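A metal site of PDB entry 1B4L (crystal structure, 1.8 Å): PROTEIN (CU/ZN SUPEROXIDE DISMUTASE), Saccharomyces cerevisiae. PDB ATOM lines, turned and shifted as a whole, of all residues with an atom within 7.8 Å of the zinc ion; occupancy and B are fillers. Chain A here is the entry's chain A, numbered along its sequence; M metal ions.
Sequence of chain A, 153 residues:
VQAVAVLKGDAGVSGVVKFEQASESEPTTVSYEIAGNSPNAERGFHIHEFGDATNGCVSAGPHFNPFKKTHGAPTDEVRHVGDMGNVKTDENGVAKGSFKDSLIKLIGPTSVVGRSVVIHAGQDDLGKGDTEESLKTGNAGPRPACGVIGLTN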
ATOM      1  N   PHE A  45     -29.902 -27.721  15.536  1.00  0.00           N
ATOM      2  CA  PHE A  45     -30.227 -26.514  14.774  1.00  0.00           C
ATOM      3  C   PHE A  45     -28.980 -25.651  14.762  1.00  0.00           C
ATOM      4  O   PHE A  45     -28.566 -25.172  15.811  1.00  0.00           O
ATOM      5  CB  PHE A  45     -31.342 -25.783  15.534  1.00  0.00           C
ATOM      6  CG  PHE A  45     -32.109 -24.782  14.713  1.00  0.00           C
ATOM      7  CD1 PHE A  45     -32.345 -24.976  13.356  1.00  0.00           C
ATOM      8  CD2 PHE A  45     -32.645 -23.660  15.323  1.00  0.00           C
ATOM      9  CE1 PHE A  45     -33.103 -24.084  12.631  1.00  0.00           C
ATOM     10  CE2 PHE A  45     -33.413 -22.749  14.600  1.00  0.00           C
ATOM     11  CZ  PHE A  45     -33.638 -22.968  13.249  1.00  0.00           C
ATOM     12  N   HIS A  46     -28.381 -25.430  13.607  1.00  0.00           N
ATOM     13  CA  HIS A  46     -27.151 -24.637  13.566  1.00  0.00           C
ATOM     14  C   HIS A  46     -27.017 -23.744  12.367  1.00  0.00           C
ATOM     15  O   HIS A  46     -27.582 -24.014  11.327  1.00  0.00           O
ATOM     16  CB  HIS A  46     -25.923 -25.553  13.521  1.00  0.00           C
ATOM     17  CG  HIS A  46     -25.966 -26.700  14.465  1.00  0.00           C
ATOM     18  ND1 HIS A  46     -25.858 -28.003  14.051  1.00  0.00           N
ATOM     19  CD2 HIS A  46     -26.172 -26.742  15.804  1.00  0.00           C
ATOM     20  CE1 HIS A  46     -26.006 -28.808  15.104  1.00  0.00           C
ATOM     21  NE2 HIS A  46     -26.200 -28.062  16.165  1.00  0.00           N
ATOM     22  N   ILE A  47     -26.148 -22.751  12.513  1.00  0.00           N
ATOM     23  CA  ILE A  47     -25.826 -21.875  11.411  1.00  0.00           C
ATOM     24  C   ILE A  47     -24.479 -22.397  10.922  1.00  0.00           C
ATOM     25  O   ILE A  47     -23.561 -22.591  11.716  1.00  0.00           O
ATOM     26  CB  ILE A  47     -25.704 -20.405  11.841  1.00  0.00           C
ATOM     27  CG1 ILE A  47     -27.093 -19.886  12.228  1.00  0.00           C
ATOM     28  CG2 ILE A  47     -25.099 -19.570  10.706  1.00  0.00           C
ATOM     29  CD1 ILE A  47     -27.120 -18.511  12.794  1.00  0.00           C
ATOM     30  N   HIS A  48     -24.424 -22.792   9.657  1.00  0.00           N
ATOM     31  CA  HIS A  48     -23.181 -23.263   9.075  1.00  0.00           C
ATOM     32  C   HIS A  48     -22.503 -22.108   8.326  1.00  0.00           C
ATOM     33  O   HIS A  48     -23.166 -21.130   7.927  1.00  0.00           O
ATOM     34  CB  HIS A  48     -23.420 -24.467   8.166  1.00  0.00           C
ATOM     35  CG  HIS A  48     -23.772 -25.713   8.926  1.00  0.00           C
ATOM     36  ND1 HIS A  48     -23.132 -26.914   8.703  1.00  0.00           N
ATOM     37  CD2 HIS A  48     -24.662 -25.941   9.916  1.00  0.00           C
ATOM     38  CE1 HIS A  48     -23.612 -27.831   9.531  1.00  0.00           C
ATOM     39  NE2 HIS A  48     -24.545 -27.256  10.275  1.00  0.00           N
ATOM     40  N   PRO A  62     -18.956 -26.440   7.715  1.00  0.00           N
ATOM     41  CA  PRO A  62     -19.008 -26.686   9.169  1.00  0.00           C
ATOM     42  C   PRO A  62     -19.790 -25.602   9.911  1.00  0.00           C
ATOM     43  O   PRO A  62     -20.296 -24.656   9.293  1.00  0.00           O
ATOM     44  CB  PRO A  62     -17.528 -26.637   9.552  1.00  0.00           C
ATOM     45  CG  PRO A  62     -17.012 -25.535   8.691  1.00  0.00           C
ATOM     46  CD  PRO A  62     -17.678 -25.795   7.340  1.00  0.00           C
ATOM     47  N   HIS A  63     -19.911 -25.739  11.221  1.00  0.00           N
ATOM     48  CA  HIS A  63     -20.629 -24.750  12.009  1.00  0.00           C
ATOM     49  C   HIS A  63     -19.852 -23.424  11.917  1.00  0.00           C
ATOM     50  O   HIS A  63     -18.622 -23.431  11.830  1.00  0.00           O
ATOM     51  CB  HIS A  63     -20.724 -25.182  13.473  1.00  0.00           C
ATOM     52  CG  HIS A  63     -21.588 -26.393  13.692  1.00  0.00           C
ATOM     53  ND1 HIS A  63     -21.721 -27.001  14.918  1.00  0.00           N
ATOM     54  CD2 HIS A  63     -22.384 -27.080  12.838  1.00  0.00           C
ATOM     55  CE1 HIS A  63     -22.561 -28.018  14.811  1.00  0.00           C
ATOM     56  NE2 HIS A  63     -22.977 -28.082  13.561  1.00  0.00           N
ATOM     57  N   PHE A  64     -20.578 -22.317  11.867  1.00  0.00           N
ATOM     58  CA  PHE A  64     -19.969 -20.994  11.794  1.00  0.00           C
ATOM     59  C   PHE A  64     -19.209 -20.849  13.114  1.00  0.00           C
ATOM     60  O   PHE A  64     -19.821 -20.795  14.172  1.00  0.00           O
ATOM     61  CB  PHE A  64     -21.044 -19.907  11.642  1.00  0.00           C
ATOM     62  CG  PHE A  64     -20.497 -18.517  11.431  1.00  0.00           C
ATOM     63  CD1 PHE A  64     -19.364 -18.307  10.635  1.00  0.00           C
ATOM     64  CD2 PHE A  64     -21.099 -17.416  12.017  1.00  0.00           C
ATOM     65  CE1 PHE A  64     -18.849 -17.037  10.449  1.00  0.00           C
ATOM     66  CE2 PHE A  64     -20.590 -16.134  11.827  1.00  0.00           C
ATOM     67  CZ  PHE A  64     -19.472 -15.943  11.046  1.00  0.00           C
ATOM     68  N   ASN A  65     -17.886 -20.772  13.027  1.00  0.00           N
ATOM     69  CA  ASN A  65     -17.004 -20.722  14.202  1.00  0.00           C
ATOM     70  C   ASN A  65     -15.854 -19.741  13.960  1.00  0.00           C
ATOM     71  O   ASN A  65     -14.686 -20.147  13.893  1.00  0.00           O
ATOM     72  CB  ASN A  65     -16.461 -22.133  14.417  1.00  0.00           C
ATOM     73  CG  ASN A  65     -15.656 -22.294  15.699  1.00  0.00           C
ATOM     74  OD1 ASN A  65     -15.958 -21.726  16.727  1.00  0.00           O
ATOM     75  ND2 ASN A  65     -14.683 -23.166  15.635  1.00  0.00           N
ATOM     76  N   LYS A  69     -13.707 -22.039  18.558  1.00  0.00           N
ATOM     77  CA  LYS A  69     -14.012 -22.676  19.834  1.00  0.00           C
ATOM     78  C   LYS A  69     -14.550 -24.063  19.516  1.00  0.00           C
ATOM     79  O   LYS A  69     -14.691 -24.403  18.335  1.00  0.00           O
ATOM     80  CB  LYS A  69     -15.099 -21.882  20.570  1.00  0.00           C
ATOM     81  CG  LYS A  69     -14.784 -20.403  20.774  1.00  0.00           C
ATOM     82  CD  LYS A  69     -13.905 -20.168  21.960  1.00  0.00           C
ATOM     83  CE  LYS A  69     -14.676 -19.427  23.069  1.00  0.00           C
ATOM     84  NZ  LYS A  69     -14.253 -17.982  23.183  1.00  0.00           N
ATOM     85  N   THR A  70     -14.822 -24.880  20.524  1.00  0.00           N
ATOM     86  CA  THR A  70     -15.391 -26.201  20.278  1.00  0.00           C
ATOM     87  C   THR A  70     -16.913 -26.098  20.339  1.00  0.00           C
ATOM     88  O   THR A  70     -17.477 -25.106  20.786  1.00  0.00           O
ATOM     89  CB  THR A  70     -14.929 -27.275  21.304  1.00  0.00           C
ATOM     90  OG1 THR A  70     -15.197 -26.830  22.631  1.00  0.00           O
ATOM     91  CG2 THR A  70     -13.453 -27.594  21.126  1.00  0.00           C
ATOM     92  N   HIS A  71     -17.568 -27.134  19.835  1.00  0.00           N
ATOM     93  CA  HIS A  71     -19.026 -27.186  19.819  1.00  0.00           C
ATOM     94  C   HIS A  71     -19.581 -27.219  21.220  1.00  0.00           C
ATOM     95  O   HIS A  71     -19.025 -27.878  22.085  1.00  0.00           O
ATOM     96  CB  HIS A  71     -19.491 -28.415  19.022  1.00  0.00           C
ATOM     97  CG  HIS A  71     -20.978 -28.549  18.946  1.00  0.00           C
ATOM     98  ND1 HIS A  71     -21.745 -27.840  18.034  1.00  0.00           N
ATOM     99  CD2 HIS A  71     -21.847 -29.257  19.708  1.00  0.00           C
ATOM    100  CE1 HIS A  71     -23.025 -28.105  18.256  1.00  0.00           C
ATOM    101  NE2 HIS A  71     -23.108 -28.962  19.263  1.00  0.00           N
ATOM    102  N   GLY A  72     -20.722 -26.563  21.418  1.00  0.00           N
ATOM    103  CA  GLY A  72     -21.351 -26.540  22.724  1.00  0.00           C
ATOM    104  C   GLY A  72     -22.822 -26.164  22.649  1.00  0.00           C
ATOM    105  O   GLY A  72     -23.421 -26.197  21.563  1.00  0.00           O
ATOM    106  N   ALA A  73     -23.417 -25.875  23.795  1.00  0.00           N
ATOM    107  CA  ALA A  73     -24.822 -25.490  23.870  1.00  0.00           C
ATOM    108  C   ALA A  73     -24.918 -23.980  23.728  1.00  0.00           C
ATOM    109  O   ALA A  73     -23.966 -23.271  24.073  1.00  0.00           O
ATOM    110  CB  ALA A  73     -25.410 -25.934  25.181  1.00  0.00           C
ATOM    111  N   ARG A  79     -18.781 -22.359  22.809  1.00  0.00           N
ATOM    112  CA  ARG A  79     -19.689 -22.868  21.778  1.00  0.00           C
ATOM    113  C   ARG A  79     -19.314 -22.181  20.472  1.00  0.00           C
ATOM    114  O   ARG A  79     -18.573 -21.191  20.484  1.00  0.00           O
ATOM    115  CB  ARG A  79     -21.151 -22.474  22.087  1.00  0.00           C
ATOM    116  CG  ARG A  79     -21.370 -20.967  22.220  1.00  0.00           C
ATOM    117  CD  ARG A  79     -22.850 -20.601  22.334  1.00  0.00           C
ATOM    118  NE  ARG A  79     -23.440 -20.218  21.056  1.00  0.00           N
ATOM    119  CZ  ARG A  79     -24.482 -19.387  20.938  1.00  0.00           C
ATOM    120  NH1 ARG A  79     -25.031 -18.858  22.024  1.00  0.00           N
ATOM    121  NH2 ARG A  79     -24.955 -19.035  19.738  1.00  0.00           N
ATOM    122  N   HIS A  80     -19.779 -22.723  19.358  1.00  0.00           N
ATOM    123  CA  HIS A  80     -19.562 -22.102  18.052  1.00  0.00           C
ATOM    124  C   HIS A  80     -20.627 -20.982  17.956  1.00  0.00           C
ATOM    125  O   HIS A  80     -21.691 -21.100  18.557  1.00  0.00           O
ATOM    126  CB  HIS A  80     -19.861 -23.110  16.930  1.00  0.00           C
ATOM    127  CG  HIS A  80     -18.928 -24.272  16.905  1.00  0.00           C
ATOM    128  ND1 HIS A  80     -19.292 -25.516  16.427  1.00  0.00           N
ATOM    129  CD2 HIS A  80     -17.611 -24.354  17.223  1.00  0.00           C
ATOM    130  CE1 HIS A  80     -18.236 -26.307  16.448  1.00  0.00           C
ATOM    131  NE2 HIS A  80     -17.208 -25.627  16.927  1.00  0.00           N
ATOM    132  N   VAL A  81     -20.358 -19.913  17.219  1.00  0.00           N
ATOM    133  CA  VAL A  81     -21.352 -18.848  17.049  1.00  0.00           C
ATOM    134  C   VAL A  81     -22.659 -19.450  16.505  1.00  0.00           C
ATOM    135  O   VAL A  81     -23.740 -19.082  16.928  1.00  0.00           O
ATOM    136  CB  VAL A  81     -20.845 -17.782  16.046  1.00  0.00           C
ATOM    137  CG1 VAL A  81     -21.957 -16.767  15.759  1.00  0.00           C
ATOM    138  CG2 VAL A  81     -19.587 -17.084  16.589  1.00  0.00           C
ATOM    139  N   GLY A  82     -22.529 -20.364  15.541  1.00  0.00           N
ATOM    140  CA  GLY A  82     -23.691 -20.988  14.919  1.00  0.00           C
ATOM    141  C   GLY A  82     -24.451 -22.035  15.718  1.00  0.00           C
ATOM    142  O   GLY A  82     -25.432 -22.601  15.218  1.00  0.00           O
ATOM    143  N   ASP A  83     -24.021 -22.287  16.955  1.00  0.00           N
ATOM    144  CA  ASP A  83     -24.640 -23.275  17.824  1.00  0.00           C
ATOM    145  C   ASP A  83     -25.953 -22.811  18.451  1.00  0.00           C
ATOM    146  O   ASP A  83     -25.985 -22.021  19.400  1.00  0.00           O
ATOM    147  CB  ASP A  83     -23.662 -23.733  18.919  1.00  0.00           C
ATOM    148  CG  ASP A  83     -22.550 -24.625  18.369  1.00  0.00           C
ATOM    149  OD1 ASP A  83     -22.611 -25.084  17.205  1.00  0.00           O
ATOM    150  OD2 ASP A  83     -21.565 -24.886  19.082  1.00  0.00           O
ATOM    151  N   MET A  84     -27.047 -23.316  17.892  1.00  0.00           N
ATOM    152  CA  MET A  84     -28.378 -22.986  18.388  1.00  0.00           C
ATOM    153  C   MET A  84     -29.016 -24.158  19.155  1.00  0.00           C
ATOM    154  O   MET A  84     -30.189 -24.105  19.501  1.00  0.00           O
ATOM    155  CB  MET A  84     -29.284 -22.481  17.250  1.00  0.00           C
ATOM    156  CG  MET A  84     -28.705 -21.285  16.497  1.00  0.00           C
ATOM    157  SD  MET A  84     -29.805 -20.576  15.287  1.00  0.00           S
ATOM    158  CE  MET A  84     -29.576 -21.728  13.946  1.00  0.00           C
ATOM    159  N   GLY A  85     -28.226 -25.200  19.426  1.00  0.00           N
ATOM    160  CA  GLY A  85     -28.708 -26.323  20.195  1.00  0.00           C
ATOM    161  C   GLY A  85     -29.662 -27.255  19.502  1.00  0.00           C
ATOM    162  O   GLY A  85     -29.400 -27.668  18.366  1.00  0.00           O
ATOM    163  N   ASP A 124     -28.601 -33.083  18.928  1.00  0.00           N
ATOM    164  CA  ASP A 124     -27.319 -32.451  19.195  1.00  0.00           C
ATOM    165  C   ASP A 124     -26.889 -32.820  20.621  1.00  0.00           C
ATOM    166  O   ASP A 124     -27.596 -32.482  21.579  1.00  0.00           O
ATOM    167  CB  ASP A 124     -27.499 -30.930  19.065  1.00  0.00           C
ATOM    168  CG  ASP A 124     -26.205 -30.151  19.183  1.00  0.00           C
ATOM    169  OD1 ASP A 124     -25.210 -30.665  19.744  1.00  0.00           O
ATOM    170  OD2 ASP A 124     -26.213 -29.001  18.708  1.00  0.00           O
ATOM    171  N   SER A 134     -18.233 -35.031  18.926  1.00  0.00           N
ATOM    172  CA  SER A 134     -19.108 -34.293  19.812  1.00  0.00           C
ATOM    173  C   SER A 134     -18.643 -32.837  19.816  1.00  0.00           C
ATOM    174  O   SER A 134     -19.448 -31.922  19.718  1.00  0.00           O
ATOM    175  CB  SER A 134     -19.014 -34.864  21.222  1.00  0.00           C
ATOM    176  OG  SER A 134     -19.878 -34.202  22.142  1.00  0.00           O
ATOM    177  N   LEU A 135     -17.326 -32.651  19.873  1.00  0.00           N
ATOM    178  CA  LEU A 135     -16.716 -31.339  19.925  1.00  0.00           C
ATOM    179  C   LEU A 135     -16.711 -30.545  18.628  1.00  0.00           C
ATOM    180  O   LEU A 135     -16.318 -29.372  18.620  1.00  0.00           O
ATOM    181  CB  LEU A 135     -15.264 -31.446  20.418  1.00  0.00           C
ATOM    182  CG  LEU A 135     -15.056 -31.934  21.847  1.00  0.00           C
ATOM    183  CD1 LEU A 135     -13.549 -31.915  22.217  1.00  0.00           C
ATOM    184  CD2 LEU A 135     -15.879 -31.075  22.814  1.00  0.00           C
ATOM    185  N   LYS A 136     -17.085 -31.184  17.529  1.00  0.00           N
ATOM    186  CA  LYS A 136     -17.107 -30.515  16.229  1.00  0.00           C
ATOM    187  C   LYS A 136     -18.529 -30.248  15.749  1.00  0.00           C
ATOM    188  O   LYS A 136     -18.896 -29.119  15.439  1.00  0.00           O
ATOM    189  CB  LYS A 136     -16.395 -31.353  15.165  1.00  0.00           C
ATOM    190  CG  LYS A 136     -14.940 -31.615  15.461  1.00  0.00           C
ATOM    191  CD  LYS A 136     -14.255 -32.278  14.274  1.00  0.00           C
ATOM    192  CE  LYS A 136     -13.297 -33.390  14.733  1.00  0.00           C
ATOM    193  NZ  LYS A 136     -14.030 -34.659  15.131  1.00  0.00           N
ATOM    194  N   THR A 137     -19.339 -31.296  15.798  1.00  0.00           N
ATOM    195  CA  THR A 137     -20.721 -31.266  15.314  1.00  0.00           C
ATOM    196  C   THR A 137     -21.776 -31.607  16.360  1.00  0.00           C
ATOM    197  O   THR A 137     -22.962 -31.338  16.137  1.00  0.00           O
ATOM    198  CB  THR A 137     -20.903 -32.325  14.185  1.00  0.00           C
ATOM    199  OG1 THR A 137     -20.888 -33.650  14.751  1.00  0.00           O
ATOM    200  CG2 THR A 137     -19.786 -32.201  13.144  1.00  0.00           C
ATOM    201  N   GLY A 138     -21.386 -32.223  17.478  1.00  0.00           N
ATOM    202  CA  GLY A 138     -22.358 -32.606  18.481  1.00  0.00           C
ATOM    203  C   GLY A 138     -23.084 -33.885  18.075  1.00  0.00           C
ATOM    204  O   GLY A 138     -24.134 -34.204  18.640  1.00  0.00           O
HETATM  205 ZN    ZN M   1     -21.241 -26.264  16.649  1.00  0.00          ZN
HETATM  206 CU    CU M   2     -25.276 -28.335  12.109  1.00  0.00          CU
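The zinc ion is bound by OD1 of Asp 83 (1.9 Å), ND1 of His 63 (1.9 Å), ND1 of His 80 (2.1 Å) and ND1 of His 71 (2.2 Å). Slightly farther from the zinc ion lies the side-chain carboxylate (OD2) of Asp 83 (2.8 Å).
Lys 136 touches the zinc ion (O to ZN, 3.9 Å). Five residues have an atom within 4 Å of the zinc ion: His 63, His 71, His 80, Asp 83 and Lys 136. The nearest printed residue that does not touch the zinc ion is Gly 72 (4.8 Å).
The backbone NH of Gly 72 sits at hydrogen-bond distance from the side-chain carboxylate of Asp 83 (3.0 Å). The backbone carbonyl oxygen of Asp 83 sits at hydrogen-bond distance from the guanidinium group of Arg 79 (3.2 Å). A ring nitrogen (ND1) of His 46 sits close to a ring nitrogen (NE2) of His 63 (2.9 Å). NE2 of His 80 sits close to O of Lys 69. A ring nitrogen (NE2) of His 71 sits at hydrogen-bond distance from the side-chain carboxylate (OD1) of Asp 124, at 2.7 Å. N of His 71 is in hydrogen-bond range of O of Leu 135 (2.8 Å).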
